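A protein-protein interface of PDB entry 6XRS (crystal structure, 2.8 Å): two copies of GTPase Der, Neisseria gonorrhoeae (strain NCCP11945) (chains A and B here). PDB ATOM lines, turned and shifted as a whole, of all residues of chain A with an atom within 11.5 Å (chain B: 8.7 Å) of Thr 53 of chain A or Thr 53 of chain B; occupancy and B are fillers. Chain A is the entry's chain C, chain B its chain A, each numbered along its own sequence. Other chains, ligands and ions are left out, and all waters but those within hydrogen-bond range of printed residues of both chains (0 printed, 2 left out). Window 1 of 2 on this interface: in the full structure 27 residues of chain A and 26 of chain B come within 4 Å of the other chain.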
ATOM      1  N   SER A  32       0.487  17.326  10.246  1.00  0.00           N
ATOM      2  CA  SER A  32       0.499  17.981  11.555  1.00  0.00           C
ATOM      3  C   SER A  32       1.920  18.182  12.054  1.00  0.00           C
ATOM      4  O   SER A  32       2.227  19.195  12.703  1.00  0.00           O
ATOM      5  CB  SER A  32      -0.321  17.194  12.566  1.00  0.00           C
ATOM      6  OG  SER A  32      -0.040  15.820  12.446  1.00  0.00           O
ATOM      7  N   PHE A  35       2.956  21.191  10.239  1.00  0.00           N
ATOM      8  CA  PHE A  35       2.214  22.337  10.761  1.00  0.00           C
ATOM      9  C   PHE A  35       2.779  22.803  12.091  1.00  0.00           C
ATOM     10  O   PHE A  35       2.872  24.010  12.351  1.00  0.00           O
ATOM     11  CB  PHE A  35       0.741  21.975  10.917  1.00  0.00           C
ATOM     12  CG  PHE A  35      -0.083  23.046  11.577  1.00  0.00           C
ATOM     13  CD1 PHE A  35      -0.651  24.058  10.824  1.00  0.00           C
ATOM     14  CD2 PHE A  35      -0.318  23.019  12.934  1.00  0.00           C
ATOM     15  CE1 PHE A  35      -1.413  25.022  11.408  1.00  0.00           C
ATOM     16  CE2 PHE A  35      -1.075  23.986  13.521  1.00  0.00           C
ATOM     17  CZ  PHE A  35      -1.625  24.993  12.755  1.00  0.00           C
ATOM     18  N   ASN A  36       3.128  21.855  12.963  1.00  0.00           N
ATOM     19  CA  ASN A  36       3.713  22.240  14.234  1.00  0.00           C
ATOM     20  C   ASN A  36       5.050  22.925  14.013  1.00  0.00           C
ATOM     21  O   ASN A  36       5.364  23.905  14.698  1.00  0.00           O
ATOM     22  CB  ASN A  36       3.839  21.027  15.153  1.00  0.00           C
ATOM     23  CG  ASN A  36       2.483  20.517  15.638  1.00  0.00           C
ATOM     24  OD1 ASN A  36       1.518  21.279  15.753  1.00  0.00           O
ATOM     25  ND2 ASN A  36       2.403  19.216  15.908  1.00  0.00           N
ATOM     26  N   THR A  39       4.221  26.531  12.831  1.00  0.00           N
ATOM     27  CA  THR A  39       3.557  27.426  13.769  1.00  0.00           C
ATOM     28  C   THR A  39       4.157  27.382  15.178  1.00  0.00           C
ATOM     29  O   THR A  39       3.575  27.964  16.101  1.00  0.00           O
ATOM     30  CB  THR A  39       2.058  27.112  13.830  1.00  0.00           C
ATOM     31  OG1 THR A  39       1.856  25.796  14.352  1.00  0.00           O
ATOM     32  CG2 THR A  39       1.429  27.188  12.436  1.00  0.00           C
ATOM     33  N   ARG A  40       5.313  26.739  15.366  1.00  0.00           N
ATOM     34  CA  ARG A  40       5.899  26.584  16.708  1.00  0.00           C
ATOM     35  C   ARG A  40       6.420  27.910  17.230  1.00  0.00           C
ATOM     36  O   ARG A  40       7.521  28.325  16.877  1.00  0.00           O
ATOM     37  CB  ARG A  40       7.039  25.556  16.720  1.00  0.00           C
ATOM     38  N   ASP A  48      -2.384  27.107  28.736  1.00  0.00           N
ATOM     39  CA  ASP A  48      -2.965  25.766  28.791  1.00  0.00           C
ATOM     40  C   ASP A  48      -2.606  25.061  30.113  1.00  0.00           C
ATOM     41  O   ASP A  48      -1.685  25.459  30.819  1.00  0.00           O
ATOM     42  CB  ASP A  48      -2.565  24.918  27.563  1.00  0.00           C
ATOM     43  CG  ASP A  48      -1.051  24.799  27.366  1.00  0.00           C
ATOM     44  OD1 ASP A  48      -0.279  25.331  28.198  1.00  0.00           O
ATOM     45  OD2 ASP A  48      -0.637  24.179  26.352  1.00  0.00           O
ATOM     46  N   LEU A  49      -3.368  24.014  30.406  1.00  0.00           N
ATOM     47  CA  LEU A  49      -3.403  23.287  31.671  1.00  0.00           C
ATOM     48  C   LEU A  49      -2.462  22.083  31.653  1.00  0.00           C
ATOM     49  O   LEU A  49      -1.964  21.667  30.607  1.00  0.00           O
ATOM     50  CB  LEU A  49      -4.832  22.837  31.909  1.00  0.00           C
ATOM     51  CG  LEU A  49      -5.880  23.915  32.082  1.00  0.00           C
ATOM     52  CD1 LEU A  49      -7.213  23.255  31.899  1.00  0.00           C
ATOM     53  CD2 LEU A  49      -5.804  24.504  33.491  1.00  0.00           C
ATOM     54  N   PRO A  50      -2.181  21.485  32.813  1.00  0.00           N
ATOM     55  CA  PRO A  50      -1.255  20.345  32.846  1.00  0.00           C
ATOM     56  C   PRO A  50      -1.861  19.095  32.228  1.00  0.00           C
ATOM     57  O   PRO A  50      -3.032  18.780  32.438  1.00  0.00           O
ATOM     58  CB  PRO A  50      -1.006  20.141  34.342  1.00  0.00           C
ATOM     59  CG  PRO A  50      -2.239  20.625  34.971  1.00  0.00           C
ATOM     60  CD  PRO A  50      -2.654  21.817  34.165  1.00  0.00           C
ATOM     61  N   GLY A  51      -1.054  18.381  31.454  1.00  0.00           N
ATOM     62  CA  GLY A  51      -1.503  17.144  30.860  1.00  0.00           C
ATOM     63  C   GLY A  51      -2.280  17.286  29.569  1.00  0.00           C
ATOM     64  O   GLY A  51      -2.532  16.279  28.900  1.00  0.00           O
ATOM     65  N   LEU A  52      -2.667  18.493  29.192  1.00  0.00           N
ATOM     66  CA  LEU A  52      -3.463  18.720  28.006  1.00  0.00           C
ATOM     67  C   LEU A  52      -2.605  19.406  26.966  1.00  0.00           C
ATOM     68  O   LEU A  52      -1.635  20.093  27.287  1.00  0.00           O
ATOM     69  CB  LEU A  52      -4.683  19.576  28.311  1.00  0.00           C
ATOM     70  CG  LEU A  52      -5.631  18.924  29.304  1.00  0.00           C
ATOM     71  CD1 LEU A  52      -6.592  19.930  29.901  1.00  0.00           C
ATOM     72  CD2 LEU A  52      -6.383  17.844  28.582  1.00  0.00           C
ATOM     73  N   THR A  53      -2.963  19.185  25.717  1.00  0.00           N
ATOM     74  CA  THR A  53      -2.342  19.851  24.597  1.00  0.00           C
ATOM     75  C   THR A  53      -3.454  20.354  23.696  1.00  0.00           C
ATOM     76  O   THR A  53      -4.398  19.618  23.414  1.00  0.00           O
ATOM     77  CB  THR A  53      -1.401  18.896  23.884  1.00  0.00           C
ATOM     78  OG1 THR A  53      -0.290  18.629  24.754  1.00  0.00           O
ATOM     79  CG2 THR A  53      -0.925  19.498  22.558  1.00  0.00           C
ATOM     80  N   ARG A  54      -3.372  21.617  23.297  1.00  0.00           N
ATOM     81  CA  ARG A  54      -4.465  22.252  22.572  1.00  0.00           C
ATOM     82  C   ARG A  54      -4.417  21.892  21.093  1.00  0.00           C
ATOM     83  O   ARG A  54      -3.414  22.139  20.425  1.00  0.00           O
ATOM     84  CB  ARG A  54      -4.391  23.764  22.772  1.00  0.00           C
ATOM     85  CG  ARG A  54      -5.511  24.525  22.104  1.00  0.00           C
ATOM     86  CD  ARG A  54      -5.815  25.865  22.763  1.00  0.00           C
ATOM     87  NE  ARG A  54      -6.440  25.700  24.065  1.00  0.00           N
ATOM     88  CZ  ARG A  54      -7.744  25.499  24.219  1.00  0.00           C
ATOM     89  NH1 ARG A  54      -8.275  25.360  25.431  1.00  0.00           N
ATOM     90  NH2 ARG A  54      -8.513  25.437  23.142  1.00  0.00           N
ATOM     91  N   ASP A  55      -5.524  21.360  20.571  1.00  0.00           N
ATOM     92  CA  ASP A  55      -5.576  20.967  19.167  1.00  0.00           C
ATOM     93  C   ASP A  55      -5.556  22.208  18.289  1.00  0.00           C
ATOM     94  O   ASP A  55      -6.287  23.172  18.543  1.00  0.00           O
ATOM     95  CB  ASP A  55      -6.837  20.158  18.874  1.00  0.00           C
ATOM     96  CG  ASP A  55      -7.068  19.052  19.887  1.00  0.00           C
ATOM     97  OD1 ASP A  55      -6.054  18.506  20.392  1.00  0.00           O
ATOM     98  OD2 ASP A  55      -8.255  18.707  20.152  1.00  0.00           O
ATOM     99  N   ARG A  56      -4.718  22.182  17.257  1.00  0.00           N
ATOM    100  CA  ARG A  56      -4.623  23.280  16.303  1.00  0.00           C
ATOM    101  C   ARG A  56      -4.498  22.688  14.915  1.00  0.00           C
ATOM    102  O   ARG A  56      -3.546  21.955  14.647  1.00  0.00           O
ATOM    103  CB  ARG A  56      -3.408  24.178  16.593  1.00  0.00           C
ATOM    104  CG  ARG A  56      -3.351  24.697  18.007  1.00  0.00           C
ATOM    105  CD  ARG A  56      -1.986  25.238  18.382  1.00  0.00           C
ATOM    106  NE  ARG A  56      -1.628  26.392  17.579  1.00  0.00           N
ATOM    107  CZ  ARG A  56      -0.600  26.425  16.737  1.00  0.00           C
ATOM    108  NH1 ARG A  56       0.177  25.353  16.599  1.00  0.00           N
ATOM    109  NH2 ARG A  56      -0.341  27.535  16.047  1.00  0.00           N
ATOM    110  N   HIS A  57      -5.410  23.028  14.020  1.00  0.00           N
ATOM    111  CA  HIS A  57      -5.182  22.728  12.620  1.00  0.00           C
ATOM    112  C   HIS A  57      -5.139  23.983  11.766  1.00  0.00           C
ATOM    113  O   HIS A  57      -5.070  23.875  10.540  1.00  0.00           O
ATOM    114  CB  HIS A  57      -6.216  21.739  12.078  1.00  0.00           C
ATOM    115  CG  HIS A  57      -7.618  22.252  12.052  1.00  0.00           C
ATOM    116  ND1 HIS A  57      -8.420  22.295  13.174  1.00  0.00           N
ATOM    117  CD2 HIS A  57      -8.377  22.718  11.032  1.00  0.00           C
ATOM    118  CE1 HIS A  57      -9.609  22.776  12.850  1.00  0.00           C
ATOM    119  NE2 HIS A  57      -9.611  23.038  11.555  1.00  0.00           N
ATOM    120  N   GLY A  75      -6.923  18.241   9.936  1.00  0.00           N
ATOM    121  CA  GLY A  75      -7.847  18.503  11.021  1.00  0.00           C
ATOM    122  C   GLY A  75      -9.314  18.536  10.641  1.00  0.00           C
ATOM    123  O   GLY A  75     -10.152  18.698  11.532  1.00  0.00           O
ATOM    124  N   ALA A 288     -18.356  23.814  21.888  1.00  0.00           N
ATOM    125  CA  ALA A 288     -17.834  22.814  20.967  1.00  0.00           C
ATOM    126  C   ALA A 288     -16.350  23.019  20.677  1.00  0.00           C
ATOM    127  O   ALA A 288     -15.793  24.096  20.898  1.00  0.00           O
ATOM    128  CB  ALA A 288     -18.616  22.831  19.644  1.00  0.00           C
ATOM    129  N   ASP A 289     -15.714  21.963  20.158  1.00  0.00           N
ATOM    130  CA  ASP A 289     -14.334  22.083  19.703  1.00  0.00           C
ATOM    131  C   ASP A 289     -14.138  23.323  18.843  1.00  0.00           C
ATOM    132  O   ASP A 289     -13.167  24.074  19.021  1.00  0.00           O
ATOM    133  CB  ASP A 289     -13.953  20.854  18.896  1.00  0.00           C
ATOM    134  CG  ASP A 289     -13.720  19.621  19.755  1.00  0.00           C
ATOM    135  OD1 ASP A 289     -13.354  19.773  20.948  1.00  0.00           O
ATOM    136  OD2 ASP A 289     -13.897  18.494  19.221  1.00  0.00           O
ATOM    137  N   ALA A 292     -13.962  26.545  20.433  1.00  0.00           N
ATOM    138  CA  ALA A 292     -12.699  26.703  21.130  1.00  0.00           C
ATOM    139  C   ALA A 292     -11.542  26.976  20.178  1.00  0.00           C
ATOM    140  O   ALA A 292     -10.666  27.790  20.503  1.00  0.00           O
ATOM    141  CB  ALA A 292     -12.412  25.472  21.982  1.00  0.00           C
ATOM    142  N   THR A 293     -11.508  26.350  18.994  1.00  0.00           N
ATOM    143  CA  THR A 293     -10.368  26.657  18.126  1.00  0.00           C
ATOM    144  C   THR A 293     -10.447  28.076  17.572  1.00  0.00           C
ATOM    145  O   THR A 293      -9.416  28.758  17.480  1.00  0.00           O
ATOM    146  CB  THR A 293     -10.276  25.690  16.965  1.00  0.00           C
ATOM    147  OG1 THR A 293     -11.506  25.757  16.255  1.00  0.00           O
ATOM    148  CG2 THR A 293     -10.004  24.271  17.438  1.00  0.00           C
ATOM    149  N   GLY A 296      -9.273  30.235  20.303  1.00  0.00           N
ATOM    150  CA  GLY A 296      -7.835  30.015  20.402  1.00  0.00           C
ATOM    151  C   GLY A 296      -7.047  30.764  19.340  1.00  0.00           C
ATOM    152  O   GLY A 296      -5.967  31.303  19.615  1.00  0.00           O
ATOM    153  N   GLU A 300      -4.111  33.570  19.935  1.00  0.00           N
ATOM    154  CA  GLU A 300      -2.776  33.550  19.346  1.00  0.00           C
ATOM    155  C   GLU A 300      -2.514  34.809  18.543  1.00  0.00           C
ATOM    156  O   GLU A 300      -1.370  35.246  18.418  1.00  0.00           O
ATOM    157  CB  GLU A 300      -2.580  32.305  18.462  1.00  0.00           C
ATOM    158  CG  GLU A 300      -2.591  30.944  19.164  1.00  0.00           C
ATOM    159  CD  GLU A 300      -2.402  29.773  18.176  1.00  0.00           C
ATOM    160  OE1 GLU A 300      -1.802  30.011  17.098  1.00  0.00           O
ATOM    161  OE2 GLU A 300      -2.853  28.623  18.460  1.00  0.00           O
ATOM    162  N   LYS A 330     -15.156  25.712  30.355  1.00  0.00           N
ATOM    163  CA  LYS A 330     -14.641  25.235  29.083  1.00  0.00           C
ATOM    164  C   LYS A 330     -13.908  26.300  28.279  1.00  0.00           C
ATOM    165  O   LYS A 330     -13.145  25.949  27.383  1.00  0.00           O
ATOM    166  CB  LYS A 330     -15.779  24.628  28.266  1.00  0.00           C
ATOM    167  CG  LYS A 330     -16.318  23.372  28.904  1.00  0.00           C
ATOM    168  CD  LYS A 330     -17.468  22.789  28.157  1.00  0.00           C
ATOM    169  CE  LYS A 330     -17.657  21.326  28.527  1.00  0.00           C
ATOM    170  NZ  LYS A 330     -18.688  20.723  27.638  1.00  0.00           N
ATOM    171  N   TYR A 332     -11.858  28.672  29.861  1.00  0.00           N
ATOM    172  CA  TYR A 332     -11.054  29.294  30.913  1.00  0.00           C
ATOM    173  C   TYR A 332     -10.029  30.267  30.353  1.00  0.00           C
ATOM    174  O   TYR A 332      -9.842  31.369  30.886  1.00  0.00           O
ATOM    175  CB  TYR A 332     -10.355  28.202  31.728  1.00  0.00           C
ATOM    176  CG  TYR A 332      -9.416  27.329  30.905  1.00  0.00           C
ATOM    177  CD1 TYR A 332      -9.895  26.204  30.221  1.00  0.00           C
ATOM    178  CD2 TYR A 332      -8.055  27.626  30.814  1.00  0.00           C
ATOM    179  CE1 TYR A 332      -9.048  25.415  29.466  1.00  0.00           C
ATOM    180  CE2 TYR A 332      -7.200  26.848  30.053  1.00  0.00           C
ATOM    181  CZ  TYR A 332      -7.698  25.740  29.381  1.00  0.00           C
ATOM    182  OH  TYR A 332      -6.850  24.951  28.626  1.00  0.00           O
ATOM    183  N   PHE A 333      -9.398  29.907  29.241  1.00  0.00           N
ATOM    184  CA  PHE A 333      -8.349  30.743  28.664  1.00  0.00           C
ATOM    185  C   PHE A 333      -8.874  32.079  28.146  1.00  0.00           C
ATOM    186  O   PHE A 333      -8.086  32.863  27.620  1.00  0.00           O
ATOM    187  CB  PHE A 333      -7.618  29.973  27.554  1.00  0.00           C
ATOM    188  CG  PHE A 333      -8.519  29.483  26.472  1.00  0.00           C
ATOM    189  CD1 PHE A 333      -9.241  28.310  26.629  1.00  0.00           C
ATOM    190  CD2 PHE A 333      -8.676  30.207  25.304  1.00  0.00           C
ATOM    191  CE1 PHE A 333     -10.109  27.871  25.636  1.00  0.00           C
ATOM    192  CE2 PHE A 333      -9.531  29.754  24.305  1.00  0.00           C
ATOM    193  CZ  PHE A 333     -10.249  28.584  24.479  1.00  0.00           C
ATOM    194  N   ASN B  36      -1.416   4.497  20.649  1.00  0.00           N
ATOM    195  CA  ASN B  36      -2.844   4.791  20.565  1.00  0.00           C
ATOM    196  C   ASN B  36      -3.610   3.584  20.053  1.00  0.00           C
ATOM    197  O   ASN B  36      -4.692   3.269  20.563  1.00  0.00           O
ATOM    198  CB  ASN B  36      -3.119   6.008  19.673  1.00  0.00           C
ATOM    199  CG  ASN B  36      -2.580   7.340  20.258  1.00  0.00           C
ATOM    200  OD1 ASN B  36      -2.433   7.539  21.489  1.00  0.00           O
ATOM    201  ND2 ASN B  36      -2.274   8.258  19.347  1.00  0.00           N
ATOM    202  N   VAL B  46     -12.652   9.768  28.705  1.00  0.00           N
ATOM    203  CA  VAL B  46     -11.806  10.733  29.407  1.00  0.00           C
ATOM    204  C   VAL B  46     -12.576  12.043  29.473  1.00  0.00           C
ATOM    205  O   VAL B  46     -13.190  12.457  28.484  1.00  0.00           O
ATOM    206  CB  VAL B  46     -10.440  10.937  28.720  1.00  0.00           C
ATOM    207  N   ASP B  48     -12.485  15.081  28.959  1.00  0.00           N
ATOM    208  CA  ASP B  48     -11.691  16.131  28.335  1.00  0.00           C
ATOM    209  C   ASP B  48     -12.563  17.293  27.865  1.00  0.00           C
ATOM    210  O   ASP B  48     -13.776  17.173  27.679  1.00  0.00           O
ATOM    211  CB  ASP B  48     -10.866  15.574  27.169  1.00  0.00           C
ATOM    212  CG  ASP B  48     -11.715  14.887  26.111  1.00  0.00           C
ATOM    213  OD1 ASP B  48     -12.961  14.884  26.240  1.00  0.00           O
ATOM    214  OD2 ASP B  48     -11.122  14.333  25.156  1.00  0.00           O
ATOM    215  N   LEU B  49     -11.910  18.423  27.681  1.00  0.00           N
ATOM    216  CA  LEU B  49     -12.487  19.726  27.400  1.00  0.00           C
ATOM    217  C   LEU B  49     -12.494  20.012  25.901  1.00  0.00           C
ATOM    218  O   LEU B  49     -11.846  19.311  25.119  1.00  0.00           O
ATOM    219  CB  LEU B  49     -11.687  20.787  28.152  1.00  0.00           C
ATOM    220  CG  LEU B  49     -11.747  20.646  29.671  1.00  0.00           C
ATOM    221  CD1 LEU B  49     -10.732  21.541  30.342  1.00  0.00           C
ATOM    222  CD2 LEU B  49     -13.149  20.969  30.181  1.00  0.00           C
ATOM    223  N   PRO B  50     -13.246  21.027  25.452  1.00  0.00           N
ATOM    224  CA  PRO B  50     -13.289  21.325  24.011  1.00  0.00           C
ATOM    225  C   PRO B  50     -11.985  21.938  23.518  1.00  0.00           C
ATOM    226  O   PRO B  50     -11.433  22.842  24.144  1.00  0.00           O
ATOM    227  CB  PRO B  50     -14.456  22.307  23.894  1.00  0.00           C
ATOM    228  CG  PRO B  50     -14.515  22.953  25.211  1.00  0.00           C
ATOM    229  CD  PRO B  50     -14.193  21.884  26.196  1.00  0.00           C
ATOM    230  N   GLY B  51     -11.503  21.451  22.374  1.00  0.00           N
ATOM    231  CA  GLY B  51     -10.291  21.953  21.765  1.00  0.00           C
ATOM    232  C   GLY B  51      -9.018  21.363  22.312  1.00  0.00           C
ATOM    233  O   GLY B  51      -7.957  21.552  21.709  1.00  0.00           O
ATOM    234  N   LEU B  52      -9.088  20.643  23.423  1.00  0.00           N
ATOM    235  CA  LEU B  52      -7.942  20.066  24.098  1.00  0.00           C
ATOM    236  C   LEU B  52      -7.976  18.561  23.945  1.00  0.00           C
ATOM    237  O   LEU B  52      -9.043  17.967  23.795  1.00  0.00           O
ATOM    238  CB  LEU B  52      -7.952  20.383  25.588  1.00  0.00           C
ATOM    239  CG  LEU B  52      -7.947  21.849  25.957  1.00  0.00           C
ATOM    240  CD1 LEU B  52      -8.356  21.969  27.399  1.00  0.00           C
ATOM    241  CD2 LEU B  52      -6.591  22.470  25.705  1.00  0.00           C
ATOM    242  N   THR B  53      -6.800  17.952  24.023  1.00  0.00           N
ATOM    243  CA  THR B  53      -6.648  16.504  24.036  1.00  0.00           C
ATOM    244  C   THR B  53      -5.733  16.095  25.180  1.00  0.00           C
ATOM    245  O   THR B  53      -4.639  16.639  25.325  1.00  0.00           O
ATOM    246  CB  THR B  53      -6.078  16.013  22.701  1.00  0.00           C
ATOM    247  OG1 THR B  53      -7.072  16.161  21.677  1.00  0.00           O
ATOM    248  CG2 THR B  53      -5.634  14.575  22.802  1.00  0.00           C
ATOM    249  N   ARG B  54      -6.160  15.135  25.985  1.00  0.00           N
ATOM    250  CA  ARG B  54      -5.365  14.772  27.145  1.00  0.00           C
ATOM    251  C   ARG B  54      -4.241  13.847  26.707  1.00  0.00           C
ATOM    252  O   ARG B  54      -4.485  12.821  26.072  1.00  0.00           O
ATOM    253  CB  ARG B  54      -6.230  14.115  28.226  1.00  0.00           C
ATOM    254  CG  ARG B  54      -5.466  13.788  29.513  1.00  0.00           C
ATOM    255  CD  ARG B  54      -6.346  13.749  30.760  1.00  0.00           C
ATOM    256  NE  ARG B  54      -6.865  15.077  31.092  1.00  0.00           N
ATOM    257  CZ  ARG B  54      -6.192  16.000  31.777  1.00  0.00           C
ATOM    258  NH1 ARG B  54      -4.967  15.722  32.201  1.00  0.00           N
ATOM    259  NH2 ARG B  54      -6.741  17.192  32.031  1.00  0.00           N
ATOM    260  N   ASP B  55      -3.014  14.230  27.046  1.00  0.00           N
ATOM    261  CA  ASP B  55      -1.818  13.462  26.704  1.00  0.00           C
ATOM    262  C   ASP B  55      -1.717  12.180  27.521  1.00  0.00           C
ATOM    263  O   ASP B  55      -1.888  12.189  28.740  1.00  0.00           O
ATOM    264  CB  ASP B  55      -0.569  14.321  26.922  1.00  0.00           C
ATOM    265  CG  ASP B  55      -0.648  15.664  26.199  1.00  0.00           C
ATOM    266  OD1 ASP B  55      -1.212  15.694  25.070  1.00  0.00           O
ATOM    267  OD2 ASP B  55      -0.174  16.689  26.763  1.00  0.00           O
ATOM    268  N   ARG B  56      -1.394  11.078  26.850  1.00  0.00           N
ATOM    269  CA  ARG B  56      -1.194   9.782  27.494  1.00  0.00           C
ATOM    270  C   ARG B  56       0.027   9.141  26.882  1.00  0.00           C
ATOM    271  O   ARG B  56       0.081   8.980  25.659  1.00  0.00           O
ATOM    272  CB  ARG B  56      -2.383   8.840  27.294  1.00  0.00           C
ATOM    273  CG  ARG B  56      -3.685   9.358  27.755  1.00  0.00           C
ATOM    274  CD  ARG B  56      -4.807   8.577  27.154  1.00  0.00           C
ATOM    275  NE  ARG B  56      -4.743   7.173  27.517  1.00  0.00           N
ATOM    276  CZ  ARG B  56      -4.614   6.197  26.628  1.00  0.00           C
ATOM    277  NH1 ARG B  56      -4.557   6.512  25.333  1.00  0.00           N
ATOM    278  NH2 ARG B  56      -4.572   4.924  27.029  1.00  0.00           N
ATOM    279  N   ASP B 289       2.611  18.515  34.597  1.00  0.00           N
ATOM    280  CA  ASP B 289       2.169  17.475  33.675  1.00  0.00           C
ATOM    281  C   ASP B 289       2.178  16.106  34.348  1.00  0.00           C
ATOM    282  O   ASP B 289       1.204  15.349  34.253  1.00  0.00           O
ATOM    283  CB  ASP B 289       3.055  17.474  32.424  1.00  0.00           C
ATOM    284  CG  ASP B 289       2.721  18.610  31.449  1.00  0.00           C
ATOM    285  OD1 ASP B 289       1.552  19.072  31.413  1.00  0.00           O
ATOM    286  OD2 ASP B 289       3.634  19.048  30.712  1.00  0.00           O
ATOM    287  N   TYR B 332      -9.451  19.470  37.185  1.00  0.00           N
ATOM    288  CA  TYR B 332     -10.914  19.469  37.095  1.00  0.00           C
ATOM    289  C   TYR B 332     -11.476  18.051  37.052  1.00  0.00           C
ATOM    290  O   TYR B 332     -12.448  17.738  37.749  1.00  0.00           O
ATOM    291  CB  TYR B 332     -11.376  20.271  35.870  1.00  0.00           C
ATOM    292  CG  TYR B 332     -10.916  19.711  34.542  1.00  0.00           C
ATOM    293  CD1 TYR B 332     -11.684  18.775  33.855  1.00  0.00           C
ATOM    294  CD2 TYR B 332      -9.711  20.114  33.975  1.00  0.00           C
ATOM    295  CE1 TYR B 332     -11.270  18.248  32.670  1.00  0.00           C
ATOM    296  CE2 TYR B 332      -9.286  19.589  32.766  1.00  0.00           C
ATOM    297  CZ  TYR B 332     -10.077  18.653  32.119  1.00  0.00           C
ATOM    298  OH  TYR B 332      -9.675  18.121  30.915  1.00  0.00           O
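O of Gly 51 of chain B sits at hydrogen-bond distance from N of Asp 55 of chain A, at 2.7 Å. The side-chain carboxylate (OD2) of Asp 55 of chain B lies within hydrogen-bond range of the side-chain hydroxyl (OG1) of Thr 53 of chain A (2.8 Å). The backbone NH of Gly 51 of chain B is in hydrogen-bond range of the side-chain carboxylate of Asp 289 of chain A, at 2.9 Å. The backbone NH (N) of Thr 53 of chain B lies within hydrogen-bond range of the backbone carbonyl oxygen (O) of Thr 53 of chain A (3.0 Å). The backbone NH (N) of Gly 51 of chain A sits at hydrogen-bond distance from the side-chain carboxylate (OD1) of Asp 289 of chain B, 2.7 Å away. The side-chain carboxylate (OD1) of Asp 55 of chain A is in hydrogen-bond range of the side-chain hydroxyl (OG1) of Thr 53 of chain B. O of Gly 51 of chain A sits at hydrogen-bond distance from N of Asp 55 of chain B, 2.8 Å away.
Hydrophobic or aromatic side chains of chain A that line the printed part of chain B: Pro 50, Leu 52, Ala 292 and Tyr 332. Of the 13 printed residues of chain B, 8 touch a printed residue of chain A. Hydrophobic or aromatic side chains of chain B within 4 Å of the printed part of chain A: Pro 50, Leu 52 and Tyr 332. Among the printed residues, no Asp or Glu carboxylate lies within 4 Å of a Lys or Arg side-chain nitrogen of the other chain.
Gly 51 of chain A touches Asp 55 of chain B, and with the chains exchanged Asp 55 of chain A touches Gly 51 of chain B. Gly 51 of chain A touches Asp 289 of chain B, and with the chains exchanged Asp 289 of chain A touches Gly 51 of chain B. Thr 53 of chain A touches its own counterpart, Thr 53 of chain B. Thr 53 of chain A touches Asp 55 of chain B, and with the chains exchanged Asp 55 of chain A touches Thr 53 of chain B.
Asp 48 of chain A touches none of the printed residues of chain B. Printed residues of chain B within 4 Å of Leu 52 of chain A: Leu 52 (3.7 Å), Thr 53 (3.6 Å), Arg 54 (3.4 Å), Asp 55 (3.7 Å) and Tyr 332 (3.7 Å). Of the printed residues of chain B, Thr 53 of chain A touches Leu 52 (3.6 Å), Thr 53 (3.0 Å) and Asp 55 (2.8 Å). Of the printed residues of chain B, Asp 55 of chain A touches Gly 51 (2.7 Å), Leu 52 (3.8 Å) and Thr 53 (2.9 Å). Gly 51 of chain B touches just these residues of chain A: Arg 54, Asp 55 and Asp 289. Of chain A, only Leu 52 (3.7 Å), Thr 53 (3.6 Å), Arg 54 (3.4 Å), Asp 55 (3.8 Å) and Tyr 332 (3.6 Å) come within 4 Å of Leu 52 of chain B. Of chain A, only Leu 52, Thr 53 and Asp 55 come within 4 Å of Thr 53 of chain B. Arg 54 of chain B touches just these residues of chain A: Pro 50, Gly 51 and Leu 52. The nearest printed residue of chain B that does not touch Tyr 332 of chain A is Leu 49 of chain B (4.3 Å).
Among the printed residues, pairs that only touch across the chains: Pro 50 of chain A with Arg 54 of chain B (3.6 Å), Pro 50 of chain A with Asp 289 of chain B (3.4 Å), Gly 51 of chain A with Arg 54 of chain B (3.7 Å), Leu 52 of chain A with Leu 52 of chain B (3.7 Å), Leu 52 of chain A with Thr 53 of chain B (3.6 Å), Leu 52 of chain A with Arg 54 of chain B (3.4 Å), Leu 52 of chain A with Asp 55 of chain B (3.7 Å), Leu 52 of chain A with Tyr 332 of chain B (3.7 Å), Thr 53 of chain A with Leu 52 of chain B (3.6 Å), Arg 54 of chain A with Gly 51 of chain B (3.6 Å), Arg 54 of chain A with Leu 52 of chain B (3.4 Å), Asp 55 of chain A with Leu 52 of chain B (3.8 Å), Ala 288 of chain A with Pro 50 of chain B (3.7 Å), Asp 289 of chain A with Pro 50 of chain B (3.4 Å), Ala 292 of chain A with Pro 50 of chain B (3.5 Å), Lys 330 of chain A with Pro 50 of chain B (3.7 Å) and Tyr 332 of chain A with Leu 52 of chain B (3.6 Å).
The guanidinium group (NH2) of Arg 54 of chain B is in hydrogen-bond range of the side-chain hydroxyl (OH) of Tyr 332 of chain B, 3.3 Å away.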
